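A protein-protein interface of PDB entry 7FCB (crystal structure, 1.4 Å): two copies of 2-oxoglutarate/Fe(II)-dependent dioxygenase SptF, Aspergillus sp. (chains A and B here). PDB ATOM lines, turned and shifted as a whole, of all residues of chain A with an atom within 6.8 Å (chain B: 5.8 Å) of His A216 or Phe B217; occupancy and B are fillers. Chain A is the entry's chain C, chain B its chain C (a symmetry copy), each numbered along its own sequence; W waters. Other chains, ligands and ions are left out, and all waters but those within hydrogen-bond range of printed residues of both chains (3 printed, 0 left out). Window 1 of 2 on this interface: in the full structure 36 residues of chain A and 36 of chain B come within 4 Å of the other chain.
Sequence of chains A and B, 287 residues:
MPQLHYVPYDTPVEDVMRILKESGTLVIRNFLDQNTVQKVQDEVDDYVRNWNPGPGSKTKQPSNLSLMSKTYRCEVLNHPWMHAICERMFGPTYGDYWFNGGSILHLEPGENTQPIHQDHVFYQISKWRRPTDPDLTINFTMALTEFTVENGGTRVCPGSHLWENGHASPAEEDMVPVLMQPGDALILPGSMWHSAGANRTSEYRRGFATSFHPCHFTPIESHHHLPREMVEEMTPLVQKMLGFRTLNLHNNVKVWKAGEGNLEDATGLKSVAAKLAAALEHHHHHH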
ATOM      1  N   TYR A  94      -7.406 -24.356 -13.297  1.00  0.00           N
ATOM      2  CA  TYR A  94      -8.782 -23.998 -13.000  1.00  0.00           C
ATOM      3  C   TYR A  94      -9.045 -23.744 -11.531  1.00  0.00           C
ATOM      4  O   TYR A  94     -10.002 -23.028 -11.212  1.00  0.00           O
ATOM      5  CB  TYR A  94      -9.723 -25.135 -13.427  1.00  0.00           C
ATOM      6  CG  TYR A  94      -9.768 -25.379 -14.904  1.00  0.00           C
ATOM      7  CD1 TYR A  94     -10.513 -24.559 -15.746  1.00  0.00           C
ATOM      8  CD2 TYR A  94      -9.059 -26.421 -15.467  1.00  0.00           C
ATOM      9  CE1 TYR A  94     -10.558 -24.790 -17.097  1.00  0.00           C
ATOM     10  CE2 TYR A  94      -9.093 -26.663 -16.823  1.00  0.00           C
ATOM     11  CZ  TYR A  94      -9.846 -25.842 -17.637  1.00  0.00           C
ATOM     12  OH  TYR A  94      -9.874 -26.078 -18.999  1.00  0.00           O
ATOM     13  N   ASP A  96     -10.614 -25.269  -8.406  1.00  0.00           N
ATOM     14  CA  ASP A  96     -11.458 -26.365  -7.965  1.00  0.00           C
ATOM     15  C   ASP A  96     -11.929 -27.226  -9.143  1.00  0.00           C
ATOM     16  O   ASP A  96     -11.971 -26.795 -10.305  1.00  0.00           O
ATOM     17  CB  ASP A  96     -12.680 -25.826  -7.222  1.00  0.00           C
ATOM     18  CG  ASP A  96     -12.369 -25.413  -5.783  1.00  0.00           C
ATOM     19  OD1 ASP A  96     -11.204 -25.597  -5.326  1.00  0.00           O
ATOM     20  OD2 ASP A  96     -13.289 -24.922  -5.121  1.00  0.00           O
ATOM     21  N   TYR A  97     -12.302 -28.454  -8.809  1.00  0.00           N
ATOM     22  CA  TYR A  97     -12.989 -29.366  -9.704  1.00  0.00           C
ATOM     23  C   TYR A  97     -14.198 -29.915  -8.954  1.00  0.00           C
ATOM     24  O   TYR A  97     -14.344 -29.730  -7.737  1.00  0.00           O
ATOM     25  CB  TYR A  97     -12.070 -30.533 -10.135  1.00  0.00           C
ATOM     26  CG  TYR A  97     -11.520 -31.267  -8.934  1.00  0.00           C
ATOM     27  CD1 TYR A  97     -10.358 -30.832  -8.286  1.00  0.00           C
ATOM     28  CD2 TYR A  97     -12.177 -32.386  -8.423  1.00  0.00           C
ATOM     29  CE1 TYR A  97      -9.882 -31.489  -7.155  1.00  0.00           C
ATOM     30  CE2 TYR A  97     -11.706 -33.039  -7.298  1.00  0.00           C
ATOM     31  CZ  TYR A  97     -10.559 -32.587  -6.673  1.00  0.00           C
ATOM     32  OH  TYR A  97     -10.090 -33.211  -5.547  1.00  0.00           O
ATOM     33  N   TRP A  98     -15.087 -30.586  -9.695  1.00  0.00           N
ATOM     34  CA  TRP A  98     -16.262 -31.194  -9.087  1.00  0.00           C
ATOM     35  C   TRP A  98     -16.729 -32.381  -9.920  1.00  0.00           C
ATOM     36  O   TRP A  98     -16.191 -32.676 -10.985  1.00  0.00           O
ATOM     37  CB  TRP A  98     -17.395 -30.187  -8.795  1.00  0.00           C
ATOM     38  CG  TRP A  98     -17.938 -29.344  -9.936  1.00  0.00           C
ATOM     39  CD1 TRP A  98     -17.413 -29.160 -11.185  1.00  0.00           C
ATOM     40  CD2 TRP A  98     -19.114 -28.531  -9.876  1.00  0.00           C
ATOM     41  NE1 TRP A  98     -18.215 -28.309 -11.918  1.00  0.00           N
ATOM     42  CE2 TRP A  98     -19.259 -27.904 -11.129  1.00  0.00           C
ATOM     43  CE3 TRP A  98     -20.072 -28.286  -8.883  1.00  0.00           C
ATOM     44  CZ2 TRP A  98     -20.300 -27.015 -11.397  1.00  0.00           C
ATOM     45  CZ3 TRP A  98     -21.107 -27.427  -9.158  1.00  0.00           C
ATOM     46  CH2 TRP A  98     -21.219 -26.808 -10.403  1.00  0.00           C
ATOM     47  N   ILE A 125     -16.124 -27.029 -26.473  1.00  0.00           N
ATOM     48  CA  ILE A 125     -14.782 -26.486 -26.321  1.00  0.00           C
ATOM     49  C   ILE A 125     -13.692 -27.516 -26.561  1.00  0.00           C
ATOM     50  O   ILE A 125     -12.516 -27.143 -26.632  1.00  0.00           O
ATOM     51  CB  ILE A 125     -14.606 -25.766 -24.967  1.00  0.00           C
ATOM     52  CG1 ILE A 125     -14.784 -26.755 -23.805  1.00  0.00           C
ATOM     53  CG2 ILE A 125     -15.572 -24.590 -24.864  1.00  0.00           C
ATOM     54  CD1 ILE A 125     -14.505 -26.153 -22.430  1.00  0.00           C
ATOM     55  N   TRP A 128     -11.632 -26.383 -29.385  1.00  0.00           N
ATOM     56  CA  TRP A 128     -10.652 -25.326 -29.171  1.00  0.00           C
ATOM     57  C   TRP A 128      -9.407 -25.832 -28.460  1.00  0.00           C
ATOM     58  O   TRP A 128      -8.347 -25.205 -28.540  1.00  0.00           O
ATOM     59  CB  TRP A 128     -11.237 -24.250 -28.251  1.00  0.00           C
ATOM     60  CG  TRP A 128     -12.546 -23.622 -28.655  1.00  0.00           C
ATOM     61  CD1 TRP A 128     -13.249 -23.797 -29.815  1.00  0.00           C
ATOM     62  CD2 TRP A 128     -13.281 -22.676 -27.874  1.00  0.00           C
ATOM     63  NE1 TRP A 128     -14.392 -23.012 -29.793  1.00  0.00           N
ATOM     64  CE2 TRP A 128     -14.431 -22.324 -28.607  1.00  0.00           C
ATOM     65  CE3 TRP A 128     -13.086 -22.112 -26.613  1.00  0.00           C
ATOM     66  CZ2 TRP A 128     -15.382 -21.415 -28.118  1.00  0.00           C
ATOM     67  CZ3 TRP A 128     -14.022 -21.206 -26.130  1.00  0.00           C
ATOM     68  CH2 TRP A 128     -15.159 -20.875 -26.881  1.00  0.00           C
ATOM     69  N   HIS A 213     -14.506 -32.938 -13.344  1.00  0.00           N
ATOM     70  CA  HIS A 213     -14.096 -31.977 -14.356  1.00  0.00           C
ATOM     71  C   HIS A 213     -13.970 -30.608 -13.708  1.00  0.00           C
ATOM     72  O   HIS A 213     -14.350 -30.426 -12.546  1.00  0.00           O
ATOM     73  CB  HIS A 213     -15.037 -32.006 -15.571  1.00  0.00           C
ATOM     74  CG  HIS A 213     -16.396 -31.434 -15.344  1.00  0.00           C
ATOM     75  ND1 HIS A 213     -17.239 -31.153 -16.397  1.00  0.00           N
ATOM     76  CD2 HIS A 213     -17.072 -31.114 -14.218  1.00  0.00           C
ATOM     77  CE1 HIS A 213     -18.365 -30.649 -15.928  1.00  0.00           C
ATOM     78  NE2 HIS A 213     -18.294 -30.615 -14.611  1.00  0.00           N
ATOM     79  N   PRO A 214     -13.396 -29.632 -14.419  1.00  0.00           N
ATOM     80  CA  PRO A 214     -13.171 -28.313 -13.817  1.00  0.00           C
ATOM     81  C   PRO A 214     -14.436 -27.671 -13.277  1.00  0.00           C
ATOM     82  O   PRO A 214     -15.530 -27.810 -13.829  1.00  0.00           O
ATOM     83  CB  PRO A 214     -12.604 -27.493 -14.978  1.00  0.00           C
ATOM     84  CG  PRO A 214     -11.852 -28.500 -15.761  1.00  0.00           C
ATOM     85  CD  PRO A 214     -12.691 -29.753 -15.705  1.00  0.00           C
ATOM     86  N   CYS A 215     -14.249 -26.886 -12.220  1.00  0.00           N
ATOM     87  CA  CYS A 215     -15.373 -26.223 -11.580  1.00  0.00           C
ATOM     88  C   CYS A 215     -16.118 -25.278 -12.506  1.00  0.00           C
ATOM     89  O   CYS A 215     -17.283 -24.982 -12.237  1.00  0.00           O
ATOM     90  CB  CYS A 215     -14.890 -25.432 -10.358  1.00  0.00           C
ATOM     91  SG  CYS A 215     -13.716 -24.058 -10.689  1.00  0.00           S
ATOM     92  N   HIS A 216     -15.474 -24.786 -13.565  1.00  0.00           N
ATOM     93  CA  HIS A 216     -16.126 -23.838 -14.462  1.00  0.00           C
ATOM     94  C   HIS A 216     -16.978 -24.501 -15.537  1.00  0.00           C
ATOM     95  O   HIS A 216     -17.519 -23.786 -16.379  1.00  0.00           O
ATOM     96  CB  HIS A 216     -15.094 -22.895 -15.082  1.00  0.00           C
ATOM     97  CG  HIS A 216     -15.579 -21.483 -15.228  1.00  0.00           C
ATOM     98  ND1 HIS A 216     -14.723 -20.422 -15.431  1.00  0.00           N
ATOM     99  CD2 HIS A 216     -16.828 -20.958 -15.185  1.00  0.00           C
ATOM    100  CE1 HIS A 216     -15.426 -19.303 -15.521  1.00  0.00           C
ATOM    101  NE2 HIS A 216     -16.707 -19.603 -15.385  1.00  0.00           N
ATOM    102  N   PHE A 217     -17.098 -25.831 -15.540  1.00  0.00           N
ATOM    103  CA  PHE A 217     -17.940 -26.534 -16.496  1.00  0.00           C
ATOM    104  C   PHE A 217     -19.120 -27.165 -15.762  1.00  0.00           C
ATOM    105  O   PHE A 217     -18.995 -27.624 -14.620  1.00  0.00           O
ATOM    106  CB  PHE A 217     -17.167 -27.657 -17.207  1.00  0.00           C
ATOM    107  CG  PHE A 217     -15.859 -27.227 -17.863  1.00  0.00           C
ATOM    108  CD1 PHE A 217     -15.594 -25.906 -18.203  1.00  0.00           C
ATOM    109  CD2 PHE A 217     -14.912 -28.198 -18.154  1.00  0.00           C
ATOM    110  CE1 PHE A 217     -14.385 -25.564 -18.805  1.00  0.00           C
ATOM    111  CE2 PHE A 217     -13.716 -27.859 -18.755  1.00  0.00           C
ATOM    112  CZ  PHE A 217     -13.453 -26.537 -19.066  1.00  0.00           C
ATOM    113  N   THR A 218     -20.261 -27.221 -16.442  1.00  0.00           N
ATOM    114  CA  THR A 218     -21.495 -27.716 -15.830  1.00  0.00           C
ATOM    115  C   THR A 218     -21.514 -29.234 -15.825  1.00  0.00           C
ATOM    116  O   THR A 218     -21.372 -29.843 -16.889  1.00  0.00           O
ATOM    117  CB  THR A 218     -22.660 -27.228 -16.671  1.00  0.00           C
ATOM    118  OG1 THR A 218     -22.538 -25.804 -16.792  1.00  0.00           O
ATOM    119  CG2 THR A 218     -23.990 -27.570 -16.003  1.00  0.00           C
ATOM    120  N   LEU A 247     -17.474 -22.545  -5.452  1.00  0.00           N
ATOM    121  CA  LEU A 247     -16.267 -23.088  -6.059  1.00  0.00           C
ATOM    122  C   LEU A 247     -15.224 -21.997  -6.240  1.00  0.00           C
ATOM    123  O   LEU A 247     -15.539 -20.893  -6.682  1.00  0.00           O
ATOM    124  CB  LEU A 247     -16.600 -23.723  -7.417  1.00  0.00           C
ATOM    125  CG  LEU A 247     -17.641 -24.849  -7.325  1.00  0.00           C
ATOM    126  CD1 LEU A 247     -18.340 -25.098  -8.650  1.00  0.00           C
ATOM    127  CD2 LEU A 247     -16.972 -26.130  -6.838  1.00  0.00           C
ATOM    128  N   LEU A 249     -11.911 -20.504  -8.029  1.00  0.00           N
ATOM    129  CA  LEU A 249     -11.003 -20.537  -9.162  1.00  0.00           C
ATOM    130  C   LEU A 249      -9.628 -20.141  -8.622  1.00  0.00           C
ATOM    131  O   LEU A 249      -9.069 -20.846  -7.775  1.00  0.00           O
ATOM    132  CB  LEU A 249     -11.500 -19.592 -10.260  1.00  0.00           C
ATOM    133  CG  LEU A 249     -12.680 -20.107 -11.111  1.00  0.00           C
ATOM    134  CD1 LEU A 249     -13.910 -20.489 -10.270  1.00  0.00           C
ATOM    135  CD2 LEU A 249     -13.081 -19.118 -12.203  1.00  0.00           C
ATOM    136  N   VAL A 253     -11.347 -15.402  -7.180  1.00  0.00           N
ATOM    137  CA  VAL A 253     -12.460 -15.575  -8.098  1.00  0.00           C
ATOM    138  C   VAL A 253     -13.227 -16.824  -7.694  1.00  0.00           C
ATOM    139  O   VAL A 253     -12.635 -17.877  -7.444  1.00  0.00           O
ATOM    140  CB  VAL A 253     -11.971 -15.646  -9.552  1.00  0.00           C
ATOM    141  CG1 VAL A 253     -13.147 -15.787 -10.490  1.00  0.00           C
ATOM    142  CG2 VAL A 253     -11.173 -14.398  -9.899  1.00  0.00           C
ATOM    143  N   VAL A 255     -17.036 -19.091  -8.455  1.00  0.00           N
ATOM    144  CA  VAL A 255     -18.288 -19.276  -9.168  1.00  0.00           C
ATOM    145  C   VAL A 255     -19.212 -20.078  -8.267  1.00  0.00           C
ATOM    146  O   VAL A 255     -18.803 -20.585  -7.215  1.00  0.00           O
ATOM    147  CB  VAL A 255     -18.111 -19.926 -10.552  1.00  0.00           C
ATOM    148  CG1 VAL A 255     -17.235 -19.036 -11.440  1.00  0.00           C
ATOM    149  CG2 VAL A 255     -17.527 -21.303 -10.424  1.00  0.00           C
ATOM    150  N   TYR B  94     -23.929 -24.289 -28.768  1.00  0.00           N
ATOM    151  CA  TYR B  94     -24.055 -24.910 -27.461  1.00  0.00           C
ATOM    152  C   TYR B  94     -25.438 -25.454 -27.173  1.00  0.00           C
ATOM    153  O   TYR B  94     -25.562 -26.358 -26.339  1.00  0.00           O
ATOM    154  CB  TYR B  94     -23.744 -23.885 -26.360  1.00  0.00           C
ATOM    155  CG  TYR B  94     -22.328 -23.400 -26.348  1.00  0.00           C
ATOM    156  CD1 TYR B  94     -21.308 -24.172 -25.798  1.00  0.00           C
ATOM    157  CD2 TYR B  94     -21.998 -22.176 -26.894  1.00  0.00           C
ATOM    158  CE1 TYR B  94     -20.013 -23.721 -25.781  1.00  0.00           C
ATOM    159  CE2 TYR B  94     -20.700 -21.712 -26.886  1.00  0.00           C
ATOM    160  CZ  TYR B  94     -19.708 -22.490 -26.327  1.00  0.00           C
ATOM    161  OH  TYR B  94     -18.404 -22.032 -26.327  1.00  0.00           O
ATOM    162  N   TRP B  98     -27.877 -20.098 -19.957  1.00  0.00           N
ATOM    163  CA  TRP B  98     -28.482 -19.801 -18.666  1.00  0.00           C
ATOM    164  C   TRP B  98     -27.818 -18.579 -18.044  1.00  0.00           C
ATOM    165  O   TRP B  98     -26.860 -18.023 -18.576  1.00  0.00           O
ATOM    166  CB  TRP B  98     -28.517 -21.013 -17.710  1.00  0.00           C
ATOM    167  CG  TRP B  98     -27.217 -21.723 -17.378  1.00  0.00           C
ATOM    168  CD1 TRP B  98     -26.000 -21.602 -17.989  1.00  0.00           C
ATOM    169  CD2 TRP B  98     -27.053 -22.714 -16.359  1.00  0.00           C
ATOM    170  NE1 TRP B  98     -25.079 -22.431 -17.383  1.00  0.00           N
ATOM    171  CE2 TRP B  98     -25.708 -23.130 -16.388  1.00  0.00           C
ATOM    172  CE3 TRP B  98     -27.914 -23.278 -15.409  1.00  0.00           C
ATOM    173  CZ2 TRP B  98     -25.218 -24.115 -15.529  1.00  0.00           C
ATOM    174  CZ3 TRP B  98     -27.424 -24.232 -14.552  1.00  0.00           C
ATOM    175  CH2 TRP B  98     -26.091 -24.636 -14.611  1.00  0.00           C
ATOM    176  N   ASN B 100     -25.689 -16.088 -15.837  1.00  0.00           N
ATOM    177  CA  ASN B 100     -24.325 -16.136 -15.330  1.00  0.00           C
ATOM    178  C   ASN B 100     -24.232 -15.387 -14.001  1.00  0.00           C
ATOM    179  O   ASN B 100     -24.031 -16.006 -12.945  1.00  0.00           O
ATOM    180  CB  ASN B 100     -23.386 -15.579 -16.412  1.00  0.00           C
ATOM    181  CG  ASN B 100     -21.930 -15.939 -16.195  1.00  0.00           C
ATOM    182  OD1 ASN B 100     -21.587 -16.734 -15.303  1.00  0.00           O
ATOM    183  ND2 ASN B 100     -21.050 -15.346 -17.022  1.00  0.00           N
ATOM    184  N   PHE B 122     -11.970 -14.139 -16.649  1.00  0.00           N
ATOM    185  CA  PHE B 122     -11.931 -15.156 -15.603  1.00  0.00           C
ATOM    186  C   PHE B 122     -12.215 -16.571 -16.109  1.00  0.00           C
ATOM    187  O   PHE B 122     -12.093 -17.516 -15.321  1.00  0.00           O
ATOM    188  CB  PHE B 122     -12.848 -14.801 -14.416  1.00  0.00           C
ATOM    189  CG  PHE B 122     -14.320 -14.980 -14.688  1.00  0.00           C
ATOM    190  CD1 PHE B 122     -15.004 -14.087 -15.497  1.00  0.00           C
ATOM    191  CD2 PHE B 122     -15.030 -16.037 -14.118  1.00  0.00           C
ATOM    192  CE1 PHE B 122     -16.363 -14.250 -15.749  1.00  0.00           C
ATOM    193  CE2 PHE B 122     -16.379 -16.193 -14.369  1.00  0.00           C
ATOM    194  CZ  PHE B 122     -17.045 -15.314 -15.178  1.00  0.00           C
ATOM    195  N   TYR B 123     -12.596 -16.744 -17.382  1.00  0.00           N
ATOM    196  CA  TYR B 123     -12.694 -18.072 -17.982  1.00  0.00           C
ATOM    197  C   TYR B 123     -11.320 -18.475 -18.482  1.00  0.00           C
ATOM    198  O   TYR B 123     -10.770 -17.821 -19.376  1.00  0.00           O
ATOM    199  CB  TYR B 123     -13.622 -18.065 -19.196  1.00  0.00           C
ATOM    200  CG  TYR B 123     -15.087 -17.826 -18.940  1.00  0.00           C
ATOM    201  CD1 TYR B 123     -15.570 -16.536 -18.800  1.00  0.00           C
ATOM    202  CD2 TYR B 123     -15.988 -18.878 -18.869  1.00  0.00           C
ATOM    203  CE1 TYR B 123     -16.907 -16.288 -18.582  1.00  0.00           C
ATOM    204  CE2 TYR B 123     -17.343 -18.636 -18.639  1.00  0.00           C
ATOM    205  CZ  TYR B 123     -17.790 -17.340 -18.506  1.00  0.00           C
ATOM    206  OH  TYR B 123     -19.119 -17.027 -18.289  1.00  0.00           O
ATOM    207  N   GLN B 124     -10.771 -19.556 -17.934  1.00  0.00           N
ATOM    208  CA  GLN B 124      -9.489 -20.027 -18.441  1.00  0.00           C
ATOM    209  C   GLN B 124      -9.573 -20.316 -19.932  1.00  0.00           C
ATOM    210  O   GLN B 124      -8.622 -20.067 -20.688  1.00  0.00           O
ATOM    211  CB  GLN B 124      -9.081 -21.290 -17.690  1.00  0.00           C
ATOM    212  CG  GLN B 124      -7.919 -21.986 -18.341  1.00  0.00           C
ATOM    213  CD  GLN B 124      -6.604 -21.266 -18.096  1.00  0.00           C
ATOM    214  OE1 GLN B 124      -6.497 -20.429 -17.196  1.00  0.00           O
ATOM    215  NE2 GLN B 124      -5.590 -21.602 -18.891  1.00  0.00           N
ATOM    216  N   ILE B 125     -10.716 -20.829 -20.388  1.00  0.00           N
ATOM    217  CA  ILE B 125     -10.883 -21.166 -21.793  1.00  0.00           C
ATOM    218  C   ILE B 125     -10.898 -19.948 -22.700  1.00  0.00           C
ATOM    219  O   ILE B 125     -10.860 -20.108 -23.925  1.00  0.00           O
ATOM    220  CB  ILE B 125     -12.112 -22.070 -22.023  1.00  0.00           C
ATOM    221  CG1 ILE B 125     -13.401 -21.338 -21.619  1.00  0.00           C
ATOM    222  CG2 ILE B 125     -11.949 -23.387 -21.272  1.00  0.00           C
ATOM    223  CD1 ILE B 125     -14.679 -22.115 -21.930  1.00  0.00           C
ATOM    224  N   ASP B 135     -18.938 -15.581 -28.245  1.00  0.00           N
ATOM    225  CA  ASP B 135     -18.534 -15.094 -26.935  1.00  0.00           C
ATOM    226  C   ASP B 135     -18.821 -16.129 -25.855  1.00  0.00           C
ATOM    227  O   ASP B 135     -19.671 -17.016 -25.999  1.00  0.00           O
ATOM    228  CB  ASP B 135     -19.264 -13.791 -26.619  1.00  0.00           C
ATOM    229  CG  ASP B 135     -18.626 -12.614 -27.295  1.00  0.00           C
ATOM    230  OD1 ASP B 135     -17.625 -12.116 -26.749  1.00  0.00           O
ATOM    231  OD2 ASP B 135     -19.102 -12.239 -28.398  1.00  0.00           O
ATOM    232  N   LEU B 136     -18.081 -16.000 -24.766  1.00  0.00           N
ATOM    233  CA  LEU B 136     -18.233 -16.881 -23.621  1.00  0.00           C
ATOM    234  C   LEU B 136     -19.353 -16.443 -22.691  1.00  0.00           C
ATOM    235  O   LEU B 136     -19.852 -17.265 -21.918  1.00  0.00           O
ATOM    236  CB  LEU B 136     -16.927 -16.927 -22.831  1.00  0.00           C
ATOM    237  CG  LEU B 136     -15.737 -17.501 -23.588  1.00  0.00           C
ATOM    238  CD1 LEU B 136     -14.462 -17.279 -22.797  1.00  0.00           C
ATOM    239  CD2 LEU B 136     -15.948 -18.968 -23.830  1.00  0.00           C
ATOM    240  N   HIS B 213     -24.712 -17.089 -20.305  1.00  0.00           N
ATOM    241  CA  HIS B 213     -23.594 -17.782 -20.925  1.00  0.00           C
ATOM    242  C   HIS B 213     -24.021 -19.204 -21.253  1.00  0.00           C
ATOM    243  O   HIS B 213     -25.104 -19.643 -20.853  1.00  0.00           O
ATOM    244  CB  HIS B 213     -22.331 -17.697 -20.056  1.00  0.00           C
ATOM    245  CG  HIS B 213     -22.355 -18.511 -18.806  1.00  0.00           C
ATOM    246  ND1 HIS B 213     -21.206 -18.738 -18.076  1.00  0.00           N
ATOM    247  CD2 HIS B 213     -23.359 -19.124 -18.140  1.00  0.00           C
ATOM    248  CE1 HIS B 213     -21.499 -19.492 -17.033  1.00  0.00           C
ATOM    249  NE2 HIS B 213     -22.794 -19.740 -17.043  1.00  0.00           N
ATOM    250  N   PRO B 214     -23.207 -19.937 -22.021  1.00  0.00           N
ATOM    251  CA  PRO B 214     -23.605 -21.287 -22.439  1.00  0.00           C
ATOM    252  C   PRO B 214     -23.934 -22.207 -21.279  1.00  0.00           C
ATOM    253  O   PRO B 214     -23.328 -22.154 -20.207  1.00  0.00           O
ATOM    254  CB  PRO B 214     -22.375 -21.790 -23.197  1.00  0.00           C
ATOM    255  CG  PRO B 214     -21.826 -20.556 -23.803  1.00  0.00           C
ATOM    256  CD  PRO B 214     -22.018 -19.483 -22.758  1.00  0.00           C
ATOM    257  N   CYS B 215     -24.862 -23.123 -21.546  1.00  0.00           N
ATOM    258  CA  CYS B 215     -25.296 -24.058 -20.522  1.00  0.00           C
ATOM    259  C   CYS B 215     -24.173 -24.936 -19.998  1.00  0.00           C
ATOM    260  O   CYS B 215     -24.300 -25.460 -18.890  1.00  0.00           O
ATOM    261  CB  CYS B 215     -26.407 -24.960 -21.073  1.00  0.00           C
ATOM    262  SG  CYS B 215     -25.953 -26.048 -22.482  1.00  0.00           S
ATOM    263  N   HIS B 216     -23.102 -25.128 -20.769  1.00  0.00           N
ATOM    264  CA  HIS B 216     -22.016 -26.000 -20.336  1.00  0.00           C
ATOM    265  C   HIS B 216     -21.000 -25.308 -19.438  1.00  0.00           C
ATOM    266  O   HIS B 216     -20.013 -25.945 -19.070  1.00  0.00           O
ATOM    267  CB  HIS B 216     -21.335 -26.642 -21.545  1.00  0.00           C
ATOM    268  CG  HIS B 216     -20.926 -28.069 -21.319  1.00  0.00           C
ATOM    269  ND1 HIS B 216     -20.621 -28.927 -22.354  1.00  0.00           N
ATOM    270  CD2 HIS B 216     -20.784 -28.789 -20.178  1.00  0.00           C
ATOM    271  CE1 HIS B 216     -20.297 -30.111 -21.860  1.00  0.00           C
ATOM    272  NE2 HIS B 216     -20.379 -30.050 -20.541  1.00  0.00           N
ATOM    273  N   PHE B 217     -21.201 -24.034 -19.090  1.00  0.00           N
ATOM    274  CA  PHE B 217     -20.309 -23.324 -18.188  1.00  0.00           C
ATOM    275  C   PHE B 217     -21.041 -23.028 -16.882  1.00  0.00           C
ATOM    276  O   PHE B 217     -22.248 -22.759 -16.869  1.00  0.00           O
ATOM    277  CB  PHE B 217     -19.852 -21.984 -18.791  1.00  0.00           C
ATOM    278  CG  PHE B 217     -19.239 -22.077 -20.185  1.00  0.00           C
ATOM    279  CD1 PHE B 217     -18.712 -23.259 -20.690  1.00  0.00           C
ATOM    280  CD2 PHE B 217     -19.183 -20.932 -20.963  1.00  0.00           C
ATOM    281  CE1 PHE B 217     -18.160 -23.293 -21.969  1.00  0.00           C
ATOM    282  CE2 PHE B 217     -18.631 -20.964 -22.228  1.00  0.00           C
ATOM    283  CZ  PHE B 217     -18.132 -22.153 -22.730  1.00  0.00           C
ATOM    284  N   THR B 218     -20.292 -23.040 -15.785  1.00  0.00           N
ATOM    285  CA  THR B 218     -20.877 -22.864 -14.454  1.00  0.00           C
ATOM    286  C   THR B 218     -21.126 -21.392 -14.174  1.00  0.00           C
ATOM    287  O   THR B 218     -20.188 -20.596 -14.261  1.00  0.00           O
ATOM    288  CB  THR B 218     -19.881 -23.381 -13.435  1.00  0.00           C
ATOM    289  OG1 THR B 218     -19.540 -24.724 -13.805  1.00  0.00           O
ATOM    290  CG2 THR B 218     -20.488 -23.378 -12.033  1.00  0.00           C
ATOM    291  N   PRO B 219     -22.347 -21.015 -13.796  1.00  0.00           N
ATOM    292  CA  PRO B 219     -22.644 -19.612 -13.480  1.00  0.00           C
ATOM    293  C   PRO B 219     -21.832 -19.052 -12.325  1.00  0.00           C
ATOM    294  O   PRO B 219     -21.515 -19.749 -11.354  1.00  0.00           O
ATOM    295  CB  PRO B 219     -24.134 -19.637 -13.118  1.00  0.00           C
ATOM    296  CG  PRO B 219     -24.677 -20.894 -13.777  1.00  0.00           C
ATOM    297  CD  PRO B 219     -23.539 -21.879 -13.709  1.00  0.00           C
HETATM  298  O   HOH W   1     -12.020 -21.056 -15.799  1.00  0.00           O
HETATM  299  O   HOH W   2     -19.120 -18.169 -14.964  1.00  0.00           O
HETATM  300  O   HOH W   3     -20.373 -31.905 -18.394  1.00  0.00           O
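O of His A216 lies within hydrogen-bond range of N of Thr B218 (2.9 Å). OG1 of Thr B218 sits at hydrogen-bond distance from O of Phe A217 (3.1 Å). OG1 of Thr A218 sits at hydrogen-bond distance from O of Phe B217, 3.1 Å away. OG1 of Thr B218 is in hydrogen-bond range of O of Cys A215, at 2.8 Å. N of Thr A218 lies within hydrogen-bond range of O of His B216 (2.9 Å). The side-chain hydroxyl of Thr A218 sits at hydrogen-bond distance from the backbone carbonyl oxygen of Cys B215 (2.8 Å).
O of Trp B98 lies within hydrogen-bond range of N of His B213. O of Asp A96 is in hydrogen-bond range of N of Cys A215 (3.0 Å). A ring nitrogen (NE2) of His A213 lies within hydrogen-bond range of the backbone carbonyl oxygen (O) of Phe A217, 3.1 Å away. ND2 of Asn B100 is in hydrogen-bond range of OH of Tyr B123, at 2.9 Å. A ring nitrogen (ND1) of His B213 is in hydrogen-bond range of the side-chain hydroxyl (OH) of Tyr B123, 2.7 Å away.
Among the printed residues, merely in contact across the chains: Tyr A94 with Gln B124 (3.8 Å), Trp A98 with Thr B218 (3.4 Å), Ile A125 with Ile B125 (3.9 Å), Trp A128 with Tyr B94 (3.5 Å), Trp A128 with Leu B136 (3.7 Å), His A216 with Phe B122 (3.5 Å), His A216 with Tyr B123 (3.4 Å), His A216 with Phe B217 (3.4 Å), Phe A217 with His B216 (3.4 Å), Thr A218 with Trp B98 (3.4 Å), Thr A218 with Thr B218 (3.7 Å), Leu A249 with Phe B122 (3.6 Å), Val A255 with Thr B218 (3.96 Å) and Val A255 with Pro B219 (3.5 Å).
His A216 touches just these residues of chain B: Phe B122 (3.5 Å), Tyr B123 (3.4 Å), Phe B217 (3.4 Å) and Thr B218 (2.9 Å). Phe B217 touches two residues of chain A. Printed residues of chain B within 4 Å of Val A255: Thr B218 (3.96 Å) and Pro B219 (3.5 Å). Of the printed residues of chain B, Cys A215 touches Thr B218. The nearest residue of chain B that does not touch His A216 is His B216 (4.3 Å). The nearest printed residue of chain A that does not touch Trp B98 is Trp A98 (6.8 Å).
Along chain A the printed residues that touch a printed residue of chain B span positions 94 to 255. Hydrophobic or aromatic side chains of chain B within 4 Å of the printed part of chain A: Tyr B94, Trp B98, Phe B122, Tyr B123, Ile B125, Leu B136, His B216 and Phe B217. Among the printed residues, no Asp or Glu carboxylate lies within 4 Å of a Lys or Arg side-chain nitrogen of the other chain.
Cys A215 touches Thr B218, and with the chains exchanged Thr A218 touches Cys B215. His A216 touches Thr B218, and with the chains exchanged Thr A218 touches His B216. Phe A217 touches Thr B218, and with the chains exchanged Thr A218 touches Phe B217. Thr A218 touches its own counterpart, Thr B218. 9 positions are printed for both chains.
Water W3 lies within hydrogen-bond range of the backbone carbonyl oxygen of Thr A218 (2.7 Å) and a ring nitrogen (NE2) of His B216 (2.8 Å). Water W2 lies within hydrogen-bond range of the backbone carbonyl oxygen (O) of Thr B218 (2.7 Å), a ring nitrogen (NE2) of His A216 (2.8 Å) and the side-chain amide oxygen (OD1) of Asn B100 (2.9 Å).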
